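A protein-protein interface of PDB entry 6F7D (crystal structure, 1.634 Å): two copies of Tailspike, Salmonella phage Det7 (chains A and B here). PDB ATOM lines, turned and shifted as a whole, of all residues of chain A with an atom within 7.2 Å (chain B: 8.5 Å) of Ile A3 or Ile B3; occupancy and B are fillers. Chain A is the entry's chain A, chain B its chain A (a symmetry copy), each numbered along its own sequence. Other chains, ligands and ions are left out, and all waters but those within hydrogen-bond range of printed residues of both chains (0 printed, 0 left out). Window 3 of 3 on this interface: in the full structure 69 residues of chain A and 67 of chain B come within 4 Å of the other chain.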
ATOM      1  N   GLY A   1     -18.450 -29.565  24.239  1.00  0.00           N
ATOM      2  CA  GLY A   1     -17.077 -29.116  24.403  1.00  0.00           C
ATOM      3  C   GLY A   1     -16.420 -28.746  23.086  1.00  0.00           C
ATOM      4  O   GLY A   1     -15.693 -29.548  22.491  1.00  0.00           O
ATOM      5  N   VAL A   2     -16.660 -27.520  22.638  1.00  0.00           N
ATOM      6  CA  VAL A   2     -16.362 -27.127  21.276  1.00  0.00           C
ATOM      7  C   VAL A   2     -15.072 -26.306  21.261  1.00  0.00           C
ATOM      8  O   VAL A   2     -14.488 -26.000  22.299  1.00  0.00           O
ATOM      9  CB  VAL A   2     -17.573 -26.380  20.632  1.00  0.00           C
ATOM     10  CG1 VAL A   2     -17.544 -24.955  20.982  1.00  0.00           C
ATOM     11  CG2 VAL A   2     -17.630 -26.576  19.111  1.00  0.00           C
ATOM     12  N   ILE A   3     -14.609 -25.963  20.053  1.00  0.00           N
ATOM     13  CA  ILE A   3     -13.286 -25.378  19.847  1.00  0.00           C
ATOM     14  C   ILE A   3     -13.125 -24.069  20.619  1.00  0.00           C
ATOM     15  O   ILE A   3     -14.085 -23.315  20.801  1.00  0.00           O
ATOM     16  CB  ILE A   3     -13.068 -25.163  18.337  1.00  0.00           C
ATOM     17  CG1 ILE A   3     -13.651 -26.338  17.545  1.00  0.00           C
ATOM     18  CG2 ILE A   3     -11.596 -24.916  18.006  1.00  0.00           C
ATOM     19  CD1 ILE A   3     -15.033 -26.052  16.975  1.00  0.00           C
ATOM     20  N   ASN A   4     -11.895 -23.798  21.073  1.00  0.00           N
ATOM     21  CA  ASN A   4     -11.572 -22.516  21.689  1.00  0.00           C
ATOM     22  C   ASN A   4     -11.645 -21.394  20.662  1.00  0.00           C
ATOM     23  O   ASN A   4     -11.385 -21.592  19.473  1.00  0.00           O
ATOM     24  CB  ASN A   4     -10.170 -22.520  22.304  1.00  0.00           C
ATOM     25  CG  ASN A   4     -10.104 -23.258  23.618  1.00  0.00           C
ATOM     26  OD1 ASN A   4     -11.130 -23.615  24.197  1.00  0.00           O
ATOM     27  ND2 ASN A   4      -8.887 -23.484  24.109  1.00  0.00           N
ATOM     28  N   PHE A   5     -11.962 -20.196  21.151  1.00  0.00           N
ATOM     29  CA  PHE A   5     -12.100 -19.028  20.292  1.00  0.00           C
ATOM     30  C   PHE A   5     -11.686 -17.788  21.074  1.00  0.00           C
ATOM     31  O   PHE A   5     -11.999 -17.663  22.260  1.00  0.00           O
ATOM     32  CB  PHE A   5     -13.539 -18.882  19.772  1.00  0.00           C
ATOM     33  CG  PHE A   5     -13.766 -17.605  19.028  1.00  0.00           C
ATOM     34  CD1 PHE A   5     -13.126 -17.379  17.816  1.00  0.00           C
ATOM     35  CD2 PHE A   5     -14.575 -16.611  19.559  1.00  0.00           C
ATOM     36  CE1 PHE A   5     -13.301 -16.185  17.112  1.00  0.00           C
ATOM     37  CE2 PHE A   5     -14.748 -15.411  18.877  1.00  0.00           C
ATOM     38  CZ  PHE A   5     -14.111 -15.192  17.650  1.00  0.00           C
ATOM     39  N   SER A   6     -10.975 -16.874  20.415  1.00  0.00           N
ATOM     40  CA  SER A   6     -10.592 -15.631  21.065  1.00  0.00           C
ATOM     41  C   SER A   6     -10.388 -14.545  20.021  1.00  0.00           C
ATOM     42  O   SER A   6      -9.831 -14.795  18.949  1.00  0.00           O
ATOM     43  CB  SER A   6      -9.314 -15.785  21.888  1.00  0.00           C
ATOM     44  OG  SER A   6      -8.871 -14.522  22.335  1.00  0.00           O
ATOM     45  N   TYR A  11      -6.280 -15.828  12.996  1.00  0.00           N
ATOM     46  CA  TYR A  11      -6.808 -16.957  12.251  1.00  0.00           C
ATOM     47  C   TYR A  11      -6.566 -16.732  10.766  1.00  0.00           C
ATOM     48  O   TYR A  11      -6.316 -15.609  10.312  1.00  0.00           O
ATOM     49  CB  TYR A  11      -8.310 -17.172  12.522  1.00  0.00           C
ATOM     50  CG  TYR A  11      -8.635 -17.485  13.970  1.00  0.00           C
ATOM     51  CD1 TYR A  11      -8.261 -18.700  14.549  1.00  0.00           C
ATOM     52  CD2 TYR A  11      -9.312 -16.560  14.769  1.00  0.00           C
ATOM     53  CE1 TYR A  11      -8.556 -18.985  15.884  1.00  0.00           C
ATOM     54  CE2 TYR A  11      -9.611 -16.839  16.087  1.00  0.00           C
ATOM     55  CZ  TYR A  11      -9.227 -18.039  16.647  1.00  0.00           C
ATOM     56  OH  TYR A  11      -9.528 -18.273  17.969  1.00  0.00           O
ATOM     57  N   VAL A  16     -13.237 -20.613  10.407  1.00  0.00           N
ATOM     58  CA  VAL A  16     -14.373 -20.286  11.269  1.00  0.00           C
ATOM     59  C   VAL A  16     -14.053 -19.071  12.133  1.00  0.00           C
ATOM     60  O   VAL A  16     -14.852 -18.135  12.246  1.00  0.00           O
ATOM     61  CB  VAL A  16     -14.745 -21.501  12.137  1.00  0.00           C
ATOM     62  CG1 VAL A  16     -15.712 -21.102  13.242  1.00  0.00           C
ATOM     63  CG2 VAL A  16     -15.327 -22.600  11.274  1.00  0.00           C
ATOM     64  N   GLY B   1     -17.840 -31.213   6.276  1.00  0.00           N
ATOM     65  CA  GLY B   1     -18.299 -31.942   7.447  1.00  0.00           C
ATOM     66  C   GLY B   1     -17.771 -31.360   8.745  1.00  0.00           C
ATOM     67  O   GLY B   1     -16.778 -31.841   9.300  1.00  0.00           O
ATOM     68  N   VAL B   2     -18.450 -30.334   9.242  1.00  0.00           N
ATOM     69  CA  VAL B   2     -17.911 -29.492  10.290  1.00  0.00           C
ATOM     70  C   VAL B   2     -18.549 -29.875  11.625  1.00  0.00           C
ATOM     71  O   VAL B   2     -19.440 -30.722  11.695  1.00  0.00           O
ATOM     72  CB  VAL B   2     -18.086 -27.980   9.938  1.00  0.00           C
ATOM     73  CG1 VAL B   2     -19.418 -27.511  10.335  1.00  0.00           C
ATOM     74  CG2 VAL B   2     -16.983 -27.111  10.559  1.00  0.00           C
ATOM     75  N   ILE B   3     -18.067 -29.255  12.708  1.00  0.00           N
ATOM     76  CA  ILE B   3     -18.404 -29.659  14.071  1.00  0.00           C
ATOM     77  C   ILE B   3     -19.910 -29.585  14.321  1.00  0.00           C
ATOM     78  O   ILE B   3     -20.608 -28.733  13.766  1.00  0.00           O
ATOM     79  CB  ILE B   3     -17.632 -28.763  15.059  1.00  0.00           C
ATOM     80  CG1 ILE B   3     -16.217 -28.496  14.536  1.00  0.00           C
ATOM     81  CG2 ILE B   3     -17.629 -29.351  16.470  1.00  0.00           C
ATOM     82  CD1 ILE B   3     -16.077 -27.153  13.839  1.00  0.00           C
ATOM     83  N   ASN B   4     -20.412 -30.492  15.170  1.00  0.00           N
ATOM     84  CA  ASN B   4     -21.801 -30.437  15.615  1.00  0.00           C
ATOM     85  C   ASN B   4     -22.037 -29.212  16.486  1.00  0.00           C
ATOM     86  O   ASN B   4     -21.142 -28.741  17.194  1.00  0.00           O
ATOM     87  CB  ASN B   4     -22.189 -31.683  16.415  1.00  0.00           C
ATOM     88  CG  ASN B   4     -22.431 -32.893  15.545  1.00  0.00           C
ATOM     89  OD1 ASN B   4     -22.507 -32.787  14.321  1.00  0.00           O
ATOM     90  ND2 ASN B   4     -22.568 -34.056  16.176  1.00  0.00           N
ATOM     91  N   PHE B   5     -23.276 -28.723  16.457  1.00  0.00           N
ATOM     92  CA  PHE B   5     -23.654 -27.539  17.213  1.00  0.00           C
ATOM     93  C   PHE B   5     -25.114 -27.662  17.631  1.00  0.00           C
ATOM     94  O   PHE B   5     -25.948 -28.133  16.856  1.00  0.00           O
ATOM     95  CB  PHE B   5     -23.435 -26.257  16.391  1.00  0.00           C
ATOM     96  CG  PHE B   5     -23.969 -25.033  17.063  1.00  0.00           C
ATOM     97  CD1 PHE B   5     -23.393 -24.575  18.242  1.00  0.00           C
ATOM     98  CD2 PHE B   5     -25.073 -24.367  16.549  1.00  0.00           C
ATOM     99  CE1 PHE B   5     -23.888 -23.447  18.903  1.00  0.00           C
ATOM    100  CE2 PHE B   5     -25.585 -23.251  17.203  1.00  0.00           C
ATOM    101  CZ  PHE B   5     -24.995 -22.788  18.385  1.00  0.00           C
ATOM    102  N   SER B   6     -25.420 -27.249  18.860  1.00  0.00           N
ATOM    103  CA  SER B   6     -26.800 -27.271  19.320  1.00  0.00           C
ATOM    104  C   SER B   6     -27.000 -26.224  20.403  1.00  0.00           C
ATOM    105  O   SER B   6     -26.139 -26.036  21.267  1.00  0.00           O
ATOM    106  CB  SER B   6     -27.200 -28.641  19.864  1.00  0.00           C
ATOM    107  OG  SER B   6     -28.469 -28.568  20.477  1.00  0.00           O
ATOM    108  N   TYR B  11     -21.641 -25.098  26.559  1.00  0.00           N
ATOM    109  CA  TYR B  11     -20.291 -24.871  26.074  1.00  0.00           C
ATOM    110  C   TYR B  11     -19.543 -24.003  27.074  1.00  0.00           C
ATOM    111  O   TYR B  11     -20.139 -23.326  27.920  1.00  0.00           O
ATOM    112  CB  TYR B  11     -20.283 -24.214  24.681  1.00  0.00           C
ATOM    113  CG  TYR B  11     -20.939 -25.053  23.602  1.00  0.00           C
ATOM    114  CD1 TYR B  11     -20.352 -26.237  23.148  1.00  0.00           C
ATOM    115  CD2 TYR B  11     -22.157 -24.667  23.035  1.00  0.00           C
ATOM    116  CE1 TYR B  11     -20.959 -27.012  22.159  1.00  0.00           C
ATOM    117  CE2 TYR B  11     -22.759 -25.427  22.051  1.00  0.00           C
ATOM    118  CZ  TYR B  11     -22.172 -26.598  21.622  1.00  0.00           C
ATOM    119  OH  TYR B  11     -22.811 -27.336  20.652  1.00  0.00           O
ATOM    120  N   GLY B  12     -18.218 -24.054  26.977  1.00  0.00           N
ATOM    121  CA  GLY B  12     -17.394 -23.153  27.754  1.00  0.00           C
ATOM    122  C   GLY B  12     -17.497 -21.725  27.252  1.00  0.00           C
ATOM    123  O   GLY B  12     -17.815 -21.465  26.092  1.00  0.00           O
ATOM    124  N   ASN B  13     -17.220 -20.785  28.153  1.00  0.00           N
ATOM    125  CA  ASN B  13     -17.365 -19.372  27.825  1.00  0.00           C
ATOM    126  C   ASN B  13     -16.435 -18.955  26.696  1.00  0.00           C
ATOM    127  O   ASN B  13     -16.720 -17.982  25.987  1.00  0.00           O
ATOM    128  CB  ASN B  13     -17.088 -18.527  29.067  1.00  0.00           C
ATOM    129  CG  ASN B  13     -17.529 -19.214  30.350  1.00  0.00           C
ATOM    130  OD1 ASN B  13     -18.548 -19.912  30.378  1.00  0.00           O
ATOM    131  ND2 ASN B  13     -16.761 -19.024  31.417  1.00  0.00           N
ATOM    132  N   ASP B  14     -15.336 -19.683  26.510  1.00  0.00           N
ATOM    133  CA  ASP B  14     -14.307 -19.383  25.524  1.00  0.00           C
ATOM    134  C   ASP B  14     -14.515 -20.090  24.200  1.00  0.00           C
ATOM    135  O   ASP B  14     -13.616 -20.068  23.355  1.00  0.00           O
ATOM    136  CB  ASP B  14     -12.937 -19.787  26.062  1.00  0.00           C
ATOM    137  CG  ASP B  14     -12.400 -18.802  27.032  1.00  0.00           C
ATOM    138  OD1 ASP B  14     -13.089 -17.788  27.265  1.00  0.00           O
ATOM    139  OD2 ASP B  14     -11.294 -19.030  27.558  1.00  0.00           O
ATOM    140  N   SER B  15     -15.649 -20.737  24.008  1.00  0.00           N
ATOM    141  CA  SER B  15     -15.795 -21.649  22.892  1.00  0.00           C
ATOM    142  C   SER B  15     -16.492 -20.990  21.704  1.00  0.00           C
ATOM    143  O   SER B  15     -17.218 -19.994  21.837  1.00  0.00           O
ATOM    144  CB  SER B  15     -16.572 -22.882  23.344  1.00  0.00           C
ATOM    145  OG  SER B  15     -17.874 -22.541  23.790  1.00  0.00           O
ATOM    146  N   VAL B  16     -16.245 -21.564  20.525  1.00  0.00           N
ATOM    147  CA  VAL B  16     -17.032 -21.228  19.338  1.00  0.00           C
ATOM    148  C   VAL B  16     -18.523 -21.358  19.634  1.00  0.00           C
ATOM    149  O   VAL B  16     -19.320 -20.470  19.308  1.00  0.00           O
ATOM    150  CB  VAL B  16     -16.621 -22.128  18.159  1.00  0.00           C
ATOM    151  CG1 VAL B  16     -17.616 -22.009  17.015  1.00  0.00           C
ATOM    152  CG2 VAL B  16     -15.221 -21.780  17.701  1.00  0.00           C
ATOM    153  N   GLY B  17     -18.916 -22.468  20.265  1.00  0.00           N
ATOM    154  CA  GLY B  17     -20.326 -22.742  20.496  1.00  0.00           C
ATOM    155  C   GLY B  17     -21.013 -21.711  21.370  1.00  0.00           C
ATOM    156  O   GLY B  17     -22.166 -21.352  21.124  1.00  0.00           O
ATOM    157  N   ALA B  18     -20.336 -21.250  22.423  1.00  0.00           N
ATOM    158  CA  ALA B  18     -20.929 -20.209  23.261  1.00  0.00           C
ATOM    159  C   ALA B  18     -21.158 -18.934  22.460  1.00  0.00           C
ATOM    160  O   ALA B  18     -22.171 -18.247  22.636  1.00  0.00           O
ATOM    161  CB  ALA B  18     -20.032 -19.903  24.462  1.00  0.00           C
ATOM    162  N   HIS B  19     -20.201 -18.583  21.601  1.00  0.00           N
ATOM    163  CA  HIS B  19     -20.360 -17.410  20.752  1.00  0.00           C
ATOM    164  C   HIS B  19     -21.560 -17.576  19.832  1.00  0.00           C
ATOM    165  O   HIS B  19     -22.409 -16.679  19.719  1.00  0.00           O
ATOM    166  CB  HIS B  19     -19.075 -17.198  19.960  1.00  0.00           C
ATOM    167  CG  HIS B  19     -19.084 -15.998  19.063  1.00  0.00           C
ATOM    168  ND1 HIS B  19     -19.642 -16.007  17.804  1.00  0.00           N
ATOM    169  CD2 HIS B  19     -18.520 -14.777  19.212  1.00  0.00           C
ATOM    170  CE1 HIS B  19     -19.447 -14.833  17.226  1.00  0.00           C
ATOM    171  NE2 HIS B  19     -18.751 -14.075  18.057  1.00  0.00           N
ATOM    172  N   LEU B  20     -21.660 -18.734  19.172  1.00  0.00           N
ATOM    173  CA  LEU B  20     -22.791 -18.986  18.285  1.00  0.00           C
ATOM    174  C   LEU B  20     -24.119 -19.032  19.032  1.00  0.00           C
ATOM    175  O   LEU B  20     -25.169 -18.782  18.429  1.00  0.00           O
ATOM    176  CB  LEU B  20     -22.593 -20.304  17.525  1.00  0.00           C
ATOM    177  CG  LEU B  20     -21.422 -20.477  16.558  1.00  0.00           C
ATOM    178  CD1 LEU B  20     -21.632 -21.785  15.792  1.00  0.00           C
ATOM    179  CD2 LEU B  20     -21.324 -19.312  15.619  1.00  0.00           C
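The backbone NH (N) of Val B16 is in hydrogen-bond range of the backbone carbonyl oxygen (O) of Ile A3 (2.8 Å). The backbone NH (N) of Phe A5 is in hydrogen-bond range of the backbone carbonyl oxygen (O) of Asp B14 (2.8 Å).
Ile A3 touches three residues of chain B. Ile B3 touches just these residues of chain A: Val A2 and Ile A3. Val A2 touches just these residues of chain B: Ile B3 (3.8 Å), Tyr B11 (3.8 Å), Ser B15 (3.3 Å), Val B16 (3.7 Å) and Gly B17 (2.9 Å). Of the printed residues of chain A, Tyr B11 touches Gly A1 (3.99 Å) and Val A2 (3.8 Å). Of the printed residues of chain A, Val B16 touches Val A2, Ile A3 and Phe A5. Of the printed residues of chain A, Asp B14 touches Asn A4 (3.6 Å) and Phe A5 (2.8 Å). Ser A6 touches none of the printed residues of chain B. Val A16 touches none of the printed residues of chain B. The nearest residue of chain B that does not touch Ile A3 is Asp B14 (4.2 Å). The nearest residue of chain A that does not touch Ile B3 is Val A16 (5.3 Å).
Among the printed residues, merely in contact across the chains: Gly A1 with Tyr B11 (3.99 Å), Val A2 with Ile B3 (3.8 Å), Val A2 with Tyr B11 (3.8 Å), Val A2 with Ser B15 (3.3 Å), Val A2 with Val B16 (3.7 Å), Val A2 with Gly B17 (2.9 Å), Ile A3 with Ile B3 (3.5 Å), Ile A3 with Ser B15 (3.2 Å), Asn A4 with Asp B14 (3.6 Å), Phe A5 with Val B16 (3.9 Å) and Phe A5 with His B19 (3.8 Å).
Val A2 touches Val B16, but with the chains exchanged Val A16 does not touch Val B2 (4.9 Å). Ile A3 touches its own counterpart, Ile B3. Ile A3 touches Val B16, but with the chains exchanged Val A16 does not touch Ile B3 (5.3 Å). Phe A5 touches Val B16, but with the chains exchanged Val A16 does not touch Phe B5 (9.8 Å). 8 positions are printed for both chains. Of the 13 pairs that touch across the chains among the printed residues, 1 has its exchanged pair printed and touching as well.
Of the 8 printed residues of chain A, 5 touch a printed residue of chain B. Hydrophobic or aromatic side chains of chain A within 4 Å of the printed part of chain B: Val A2, Ile A3 and Phe A5. Printed residues of chain B that touch a printed residue of chain A: Ile B3, Tyr B11, Asp B14, Ser B15, Val B16, Gly B17 and His B19. Hydrophobic or aromatic side chains of chain B within 4 Å of the printed part of chain A: Ile B3, Tyr B11, Val B16 and His B19. Among the printed residues, no Asp or Glu carboxylate lies within 4 Å of a Lys or Arg side-chain nitrogen of the other chain.
The backbone NH (N) of Ser B6 is in hydrogen-bond range of the side-chain hydroxyl (OH) of Tyr B11 (3.2 Å). The side-chain hydroxyl (OG) of Ser B15 sits at hydrogen-bond distance from the backbone carbonyl oxygen (O) of Gly B12, 2.5 Å away. The backbone NH (N) of Ala B18 is in hydrogen-bond range of the side-chain hydroxyl (OG) of Ser B15 (3.1 Å).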
